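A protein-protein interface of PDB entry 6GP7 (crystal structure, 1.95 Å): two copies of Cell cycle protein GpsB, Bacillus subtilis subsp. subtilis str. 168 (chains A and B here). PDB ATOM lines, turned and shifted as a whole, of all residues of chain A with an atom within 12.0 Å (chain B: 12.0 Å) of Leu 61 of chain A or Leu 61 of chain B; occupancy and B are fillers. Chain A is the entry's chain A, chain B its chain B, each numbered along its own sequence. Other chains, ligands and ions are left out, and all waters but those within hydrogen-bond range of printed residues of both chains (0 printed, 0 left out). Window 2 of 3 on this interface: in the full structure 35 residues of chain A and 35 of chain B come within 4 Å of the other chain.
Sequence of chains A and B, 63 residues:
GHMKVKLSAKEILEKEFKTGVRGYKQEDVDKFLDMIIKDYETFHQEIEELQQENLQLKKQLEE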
ATOM      1  N   LEU A  50       6.435  -0.210 -13.101  1.00  0.00           N
ATOM      2  CA  LEU A  50       5.969  -1.155 -12.088  1.00  0.00           C
ATOM      3  C   LEU A  50       4.516  -0.901 -11.697  1.00  0.00           C
ATOM      4  O   LEU A  50       3.762  -1.848 -11.452  1.00  0.00           O
ATOM      5  CB  LEU A  50       6.872  -1.086 -10.857  1.00  0.00           C
ATOM      6  CG  LEU A  50       8.190  -1.830 -11.033  1.00  0.00           C
ATOM      7  CD1 LEU A  50       9.226  -1.351 -10.016  1.00  0.00           C
ATOM      8  CD2 LEU A  50       7.929  -3.324 -10.922  1.00  0.00           C
ATOM      9  N   GLN A  52       2.080   0.439 -13.593  1.00  0.00           N
ATOM     10  CA  GLN A  52       1.221  -0.046 -14.665  1.00  0.00           C
ATOM     11  C   GLN A  52       1.123  -1.560 -14.633  1.00  0.00           C
ATOM     12  O   GLN A  52       0.038  -2.126 -14.808  1.00  0.00           O
ATOM     13  CB  GLN A  52       1.745   0.420 -16.022  1.00  0.00           C
ATOM     14  CG  GLN A  52       1.700   1.920 -16.210  1.00  0.00           C
ATOM     15  CD  GLN A  52       0.348   2.502 -15.842  1.00  0.00           C
ATOM     16  OE1 GLN A  52      -0.680   2.137 -16.423  1.00  0.00           O
ATOM     17  NE2 GLN A  52       0.338   3.404 -14.858  1.00  0.00           N
ATOM     18  N   GLU A  53       2.250  -2.234 -14.401  1.00  0.00           N
ATOM     19  CA  GLU A  53       2.245  -3.691 -14.389  1.00  0.00           C
ATOM     20  C   GLU A  53       1.429  -4.233 -13.225  1.00  0.00           C
ATOM     21  O   GLU A  53       0.626  -5.156 -13.401  1.00  0.00           O
ATOM     22  CB  GLU A  53       3.678  -4.213 -14.331  1.00  0.00           C
ATOM     23  CG  GLU A  53       3.746  -5.726 -14.340  1.00  0.00           C
ATOM     24  CD  GLU A  53       5.152  -6.227 -14.577  1.00  0.00           C
ATOM     25  OE1 GLU A  53       6.024  -5.400 -14.930  1.00  0.00           O
ATOM     26  OE2 GLU A  53       5.381  -7.445 -14.418  1.00  0.00           O
ATOM     27  N   ASN A  54       1.618  -3.674 -12.027  1.00  0.00           N
ATOM     28  CA  ASN A  54       0.836  -4.117 -10.878  1.00  0.00           C
ATOM     29  C   ASN A  54      -0.644  -3.823 -11.071  1.00  0.00           C
ATOM     30  O   ASN A  54      -1.494  -4.620 -10.659  1.00  0.00           O
ATOM     31  CB  ASN A  54       1.357  -3.461  -9.604  1.00  0.00           C
ATOM     32  CG  ASN A  54       2.707  -4.003  -9.187  1.00  0.00           C
ATOM     33  OD1 ASN A  54       3.276  -4.858  -9.857  1.00  0.00           O
ATOM     34  ND2 ASN A  54       3.229  -3.503  -8.078  1.00  0.00           N
ATOM     35  N   LEU A  55      -0.975  -2.692 -11.701  1.00  0.00           N
ATOM     36  CA  LEU A  55      -2.372  -2.401 -12.005  1.00  0.00           C
ATOM     37  C   LEU A  55      -2.958  -3.464 -12.924  1.00  0.00           C
ATOM     38  O   LEU A  55      -4.039  -3.999 -12.656  1.00  0.00           O
ATOM     39  CB  LEU A  55      -2.507  -1.014 -12.635  1.00  0.00           C
ATOM     40  N   GLN A  56      -2.251  -3.791 -14.011  1.00  0.00           N
ATOM     41  CA  GLN A  56      -2.740  -4.818 -14.925  1.00  0.00           C
ATOM     42  C   GLN A  56      -2.871  -6.161 -14.225  1.00  0.00           C
ATOM     43  O   GLN A  56      -3.846  -6.887 -14.440  1.00  0.00           O
ATOM     44  CB  GLN A  56      -1.817  -4.938 -16.137  1.00  0.00           C
ATOM     45  N   LEU A  57      -1.902  -6.507 -13.376  1.00  0.00           N
ATOM     46  CA  LEU A  57      -1.983  -7.765 -12.640  1.00  0.00           C
ATOM     47  C   LEU A  57      -3.165  -7.760 -11.681  1.00  0.00           C
ATOM     48  O   LEU A  57      -3.889  -8.759 -11.570  1.00  0.00           O
ATOM     49  CB  LEU A  57      -0.680  -8.022 -11.882  1.00  0.00           C
ATOM     50  CG  LEU A  57       0.576  -8.268 -12.719  1.00  0.00           C
ATOM     51  CD1 LEU A  57       1.815  -8.246 -11.835  1.00  0.00           C
ATOM     52  CD2 LEU A  57       0.476  -9.573 -13.475  1.00  0.00           C
ATOM     53  N   LYS A  58      -3.379  -6.641 -10.980  1.00  0.00           N
ATOM     54  CA  LYS A  58      -4.498  -6.544 -10.050  1.00  0.00           C
ATOM     55  C   LYS A  58      -5.824  -6.693 -10.769  1.00  0.00           C
ATOM     56  O   LYS A  58      -6.789  -7.205 -10.193  1.00  0.00           O
ATOM     57  CB  LYS A  58      -4.456  -5.212  -9.295  1.00  0.00           C
ATOM     58  CG  LYS A  58      -3.430  -5.142  -8.177  1.00  0.00           C
ATOM     59  CD  LYS A  58      -3.316  -3.721  -7.634  1.00  0.00           C
ATOM     60  CE  LYS A  58      -2.144  -3.573  -6.680  1.00  0.00           C
ATOM     61  NZ  LYS A  58      -1.906  -2.147  -6.295  1.00  0.00           N
ATOM     62  N   LYS A  59      -5.893  -6.259 -12.026  1.00  0.00           N
ATOM     63  CA  LYS A  59      -7.105  -6.467 -12.803  1.00  0.00           C
ATOM     64  C   LYS A  59      -7.349  -7.948 -13.075  1.00  0.00           C
ATOM     65  O   LYS A  59      -8.504  -8.387 -13.103  1.00  0.00           O
ATOM     66  CB  LYS A  59      -7.028  -5.677 -14.110  1.00  0.00           C
ATOM     67  N   GLN A  60      -6.283  -8.734 -13.256  1.00  0.00           N
ATOM     68  CA  GLN A  60      -6.459 -10.148 -13.572  1.00  0.00           C
ATOM     69  C   GLN A  60      -6.977 -10.941 -12.380  1.00  0.00           C
ATOM     70  O   GLN A  60      -7.635 -11.971 -12.567  1.00  0.00           O
ATOM     71  CB  GLN A  60      -5.144 -10.754 -14.062  1.00  0.00           C
ATOM     72  CG  GLN A  60      -4.576 -10.103 -15.309  1.00  0.00           C
ATOM     73  CD  GLN A  60      -3.385 -10.862 -15.863  1.00  0.00           C
ATOM     74  OE1 GLN A  60      -3.367 -12.094 -15.861  1.00  0.00           O
ATOM     75  NE2 GLN A  60      -2.382 -10.132 -16.332  1.00  0.00           N
ATOM     76  N   LEU A  61      -6.697 -10.495 -11.161  1.00  0.00           N
ATOM     77  CA  LEU A  61      -7.130 -11.225  -9.974  1.00  0.00           C
ATOM     78  C   LEU A  61      -8.596 -10.957  -9.618  1.00  0.00           C
ATOM     79  O   LEU A  61      -9.096  -9.842  -9.777  1.00  0.00           O
ATOM     80  CB  LEU A  61      -6.236 -10.878  -8.786  1.00  0.00           C
ATOM     81  CG  LEU A  61      -4.846 -11.511  -8.792  1.00  0.00           C
ATOM     82  CD1 LEU A  61      -4.095 -11.130  -7.536  1.00  0.00           C
ATOM     83  CD2 LEU A  61      -4.944 -13.013  -8.904  1.00  0.00           C
ATOM     84  N   GLN B  52       8.126  -6.117  -4.830  1.00  0.00           N
ATOM     85  CA  GLN B  52       7.598  -7.185  -3.987  1.00  0.00           C
ATOM     86  C   GLN B  52       6.115  -7.414  -4.243  1.00  0.00           C
ATOM     87  O   GLN B  52       5.655  -8.561  -4.261  1.00  0.00           O
ATOM     88  CB  GLN B  52       7.838  -6.870  -2.511  1.00  0.00           C
ATOM     89  CG  GLN B  52       9.295  -6.944  -2.106  1.00  0.00           C
ATOM     90  CD  GLN B  52      10.033  -8.080  -2.791  1.00  0.00           C
ATOM     91  OE1 GLN B  52       9.652  -9.249  -2.674  1.00  0.00           O
ATOM     92  NE2 GLN B  52      11.096  -7.741  -3.517  1.00  0.00           N
ATOM     93  N   GLU B  53       5.345  -6.339  -4.416  1.00  0.00           N
ATOM     94  CA  GLU B  53       3.934  -6.511  -4.742  1.00  0.00           C
ATOM     95  C   GLU B  53       3.780  -7.227  -6.076  1.00  0.00           C
ATOM     96  O   GLU B  53       3.001  -8.175  -6.193  1.00  0.00           O
ATOM     97  CB  GLU B  53       3.219  -5.162  -4.776  1.00  0.00           C
ATOM     98  CG  GLU B  53       1.739  -5.283  -5.128  1.00  0.00           C
ATOM     99  CD  GLU B  53       1.071  -3.942  -5.349  1.00  0.00           C
ATOM    100  OE1 GLU B  53       1.427  -3.253  -6.329  1.00  0.00           O
ATOM    101  OE2 GLU B  53       0.194  -3.573  -4.539  1.00  0.00           O
ATOM    102  N   ASN B  54       4.516  -6.769  -7.093  1.00  0.00           N
ATOM    103  CA  ASN B  54       4.521  -7.405  -8.408  1.00  0.00           C
ATOM    104  C   ASN B  54       4.779  -8.900  -8.297  1.00  0.00           C
ATOM    105  O   ASN B  54       4.102  -9.716  -8.932  1.00  0.00           O
ATOM    106  CB  ASN B  54       5.588  -6.735  -9.282  1.00  0.00           C
ATOM    107  CG  ASN B  54       5.551  -7.191 -10.731  1.00  0.00           C
ATOM    108  OD1 ASN B  54       4.726  -6.730 -11.515  1.00  0.00           O
ATOM    109  ND2 ASN B  54       6.469  -8.076 -11.099  1.00  0.00           N
ATOM    110  N   LEU B  55       5.757  -9.278  -7.478  1.00  0.00           N
ATOM    111  CA  LEU B  55       6.066 -10.691  -7.315  1.00  0.00           C
ATOM    112  C   LEU B  55       4.911 -11.440  -6.661  1.00  0.00           C
ATOM    113  O   LEU B  55       4.559 -12.545  -7.093  1.00  0.00           O
ATOM    114  CB  LEU B  55       7.344 -10.851  -6.502  1.00  0.00           C
ATOM    115  CG  LEU B  55       7.883 -12.277  -6.469  1.00  0.00           C
ATOM    116  CD1 LEU B  55       8.321 -12.677  -7.870  1.00  0.00           C
ATOM    117  CD2 LEU B  55       9.028 -12.395  -5.478  1.00  0.00           C
ATOM    118  N   GLN B  56       4.301 -10.854  -5.623  1.00  0.00           N
ATOM    119  CA  GLN B  56       3.206 -11.527  -4.930  1.00  0.00           C
ATOM    120  C   GLN B  56       1.978 -11.649  -5.822  1.00  0.00           C
ATOM    121  O   GLN B  56       1.288 -12.675  -5.793  1.00  0.00           O
ATOM    122  CB  GLN B  56       2.859 -10.790  -3.637  1.00  0.00           C
ATOM    123  N   LEU B  57       1.685 -10.617  -6.622  1.00  0.00           N
ATOM    124  CA  LEU B  57       0.559 -10.707  -7.550  1.00  0.00           C
ATOM    125  C   LEU B  57       0.793 -11.804  -8.579  1.00  0.00           C
ATOM    126  O   LEU B  57      -0.120 -12.577  -8.895  1.00  0.00           O
ATOM    127  CB  LEU B  57       0.335  -9.362  -8.245  1.00  0.00           C
ATOM    128  CG  LEU B  57      -0.160  -8.207  -7.378  1.00  0.00           C
ATOM    129  CD1 LEU B  57      -0.002  -6.883  -8.111  1.00  0.00           C
ATOM    130  CD2 LEU B  57      -1.613  -8.434  -6.990  1.00  0.00           C
ATOM    131  N   LYS B  58       2.016 -11.885  -9.108  1.00  0.00           N
ATOM    132  CA  LYS B  58       2.345 -12.939 -10.058  1.00  0.00           C
ATOM    133  C   LYS B  58       2.135 -14.317  -9.440  1.00  0.00           C
ATOM    134  O   LYS B  58       1.488 -15.186 -10.040  1.00  0.00           O
ATOM    135  CB  LYS B  58       3.786 -12.766 -10.549  1.00  0.00           C
ATOM    136  CG  LYS B  58       3.954 -11.679 -11.601  1.00  0.00           C
ATOM    137  CD  LYS B  58       5.406 -11.563 -12.043  1.00  0.00           C
ATOM    138  CE  LYS B  58       5.580 -10.540 -13.155  1.00  0.00           C
ATOM    139  NZ  LYS B  58       7.026 -10.306 -13.442  1.00  0.00           N
ATOM    140  N   LYS B  59       2.653 -14.528  -8.225  1.00  0.00           N
ATOM    141  CA  LYS B  59       2.520 -15.836  -7.585  1.00  0.00           C
ATOM    142  C   LYS B  59       1.056 -16.221  -7.400  1.00  0.00           C
ATOM    143  O   LYS B  59       0.681 -17.381  -7.614  1.00  0.00           O
ATOM    144  CB  LYS B  59       3.252 -15.849  -6.244  1.00  0.00           C
ATOM    145  N   GLN B  60       0.210 -15.261  -7.016  1.00  0.00           N
ATOM    146  CA  GLN B  60      -1.207 -15.547  -6.829  1.00  0.00           C
ATOM    147  C   GLN B  60      -1.923 -15.839  -8.140  1.00  0.00           C
ATOM    148  O   GLN B  60      -2.994 -16.453  -8.122  1.00  0.00           O
ATOM    149  CB  GLN B  60      -1.889 -14.384  -6.107  1.00  0.00           C
ATOM    150  CG  GLN B  60      -1.560 -14.314  -4.613  1.00  0.00           C
ATOM    151  CD  GLN B  60      -1.896 -12.970  -3.999  1.00  0.00           C
ATOM    152  OE1 GLN B  60      -2.400 -12.075  -4.676  1.00  0.00           O
ATOM    153  NE2 GLN B  60      -1.613 -12.819  -2.708  1.00  0.00           N
ATOM    154  N   LEU B  61      -1.361 -15.422  -9.273  1.00  0.00           N
ATOM    155  CA  LEU B  61      -1.980 -15.726 -10.557  1.00  0.00           C
ATOM    156  C   LEU B  61      -1.704 -17.158 -10.992  1.00  0.00           C
ATOM    157  O   LEU B  61      -2.565 -17.798 -11.606  1.00  0.00           O
ATOM    158  CB  LEU B  61      -1.494 -14.742 -11.618  1.00  0.00           C
ATOM    159  CG  LEU B  61      -2.256 -13.417 -11.623  1.00  0.00           C
ATOM    160  CD1 LEU B  61      -1.495 -12.369 -12.414  1.00  0.00           C
ATOM    161  CD2 LEU B  61      -3.651 -13.614 -12.206  1.00  0.00           C
ATOM    162  N   GLU B  62      -0.526 -17.685 -10.686  1.00  0.00           N
ATOM    163  CA  GLU B  62      -0.217 -19.045 -11.104  1.00  0.00           C
ATOM    164  C   GLU B  62      -0.688 -20.067 -10.076  1.00  0.00           C
ATOM    165  O   GLU B  62      -1.436 -19.731  -9.158  1.00  0.00           O
ATOM    166  CB  GLU B  62       1.281 -19.200 -11.365  1.00  0.00           C
ATOM    167  CG  GLU B  62       2.179 -18.831 -10.207  1.00  0.00           C
ATOM    168  CD  GLU B  62       3.646 -19.080 -10.524  1.00  0.00           C
ATOM    169  OE1 GLU B  62       3.939 -20.026 -11.282  1.00  0.00           O
ATOM    170  OE2 GLU B  62       4.508 -18.330 -10.025  1.00  0.00           O
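OE1 of Glu 53 of chain B lies within hydrogen-bond range of ND2 of Asn 54 of chain A, 2.5 Å away.
OE2 of Glu 53 of chain B is in salt-bridge range of NZ of Lys 58 of chain A (3.1 Å).
OD1 of Asn 54 of chain B sits close to OE2 of Glu 53 of chain A, 3.1 Å away.
OD1 of Asn 54 of chain A lies close to OD1 of Asn 54 of chain B, 2.9 Å away.
The side-chain carboxylate (OE2) of Glu 53 of chain A lies within salt-bridge range of the side-chain amino group (NZ) of Lys 58 of chain B (3.4 Å).
The side-chain amide nitrogen of Asn 54 of chain B sits close to the side-chain amino group of Lys 58 of chain B.
The side-chain amide oxygen of Asn 54 of chain A sits close to the backbone carbonyl oxygen of Leu 50 of chain A.
Asn 54 of chain A touches Leu 57 of chain B (O to CD1, 3.7 Å).
Leu 57 of chain A touches Asn 54 of chain B (CD1 to OD1, 3.3 Å).
Leu 57 of chain B touches Leu 57 of chain A (CD1 to CB, 3.997 Å).
Leu 57 of chain A touches Leu 61 of chain B.
CG of Lys 58 of chain A touches CD1 of Leu 57 of chain B (3.8 Å).
CD2 of Leu 61 of chain B touches CB of Gln 60 of chain A, at 3.7 Å.
CD1 of Leu 61 of chain A touches CD2 of Leu 57 of chain B (3.7 Å).
OE1 of Gln 60 of chain B touches CD1 of Leu 61 of chain A (3.5 Å).
CD2 of Leu 61 of chain B touches CD2 of Leu 61 of chain A (3.6 Å).
Printed residues of chain B within 4 Å of Glu 53 of chain A: Asn 54 (3.1 Å) and Lys 58 (3.3 Å).
Printed residues of chain B within 4 Å of Asn 54 of chain A: Glu 53 (2.5 Å), Asn 54 (2.9 Å) and Leu 57 (3.7 Å).
Of the printed residues of chain B, Lys 58 of chain A touches Glu 53 and Leu 57.
Gln 60 of chain A touches one residue of chain B.
Of the printed residues of chain B, Leu 61 of chain A touches Leu 57 (3.7 Å), Gln 60 (3.5 Å) and Leu 61 (3.6 Å).
Of the printed residues of chain A, Asn 54 of chain B touches Glu 53, Asn 54 and Leu 57.
Of the printed residues of chain A, Lys 58 of chain B touches Glu 53 (3.3 Å).
Lys 59 of chain B touches none of the printed residues of chain A.
Leu 61 of chain B touches just these residues of chain A: Leu 57, Gln 60 and Leu 61.
No residue of chain A comes within 4 Å of Glu 62 of chain B.
The nearest residue of chain B that does not touch Leu 61 of chain A is Gln 56 of chain B (5.9 Å).
The nearest residue of chain A that does not touch Leu 61 of chain B is Lys 58 of chain A (6.2 Å).
The nearest printed residue of chain B that does not touch Glu 53 of chain A is Leu 57 of chain B (5.6 Å).
Of the 11 printed residues of chain B, 6 touch a printed residue of chain A.
Hydrophobic or aromatic side chains of chain B that line the printed part of chain A: Leu 57 and Leu 61.
Among the printed residues, 14 pairs touch across the chains.
Glu 53 of chain A touches Asn 54 of chain B, and with the chains exchanged Asn 54 of chain A touches Glu 53 of chain B.
Asn 54 of chain B touches its own counterpart, Asn 54 of chain A.
Leu 57 of chain A touches Leu 61 of chain B, and with the chains exchanged Leu 61 of chain A touches Leu 57 of chain B.
Gln 60 of chain A touches Leu 61 of chain B, and with the chains exchanged Leu 61 of chain A touches Gln 60 of chain B.
Positions printed for both chains: 52, 53, 54, 55, 56, 57, 58, 59, 60 and 61.
Of the 14 pairs that touch across the chains among the printed residues, 13 have their exchanged pair printed and touching as well.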
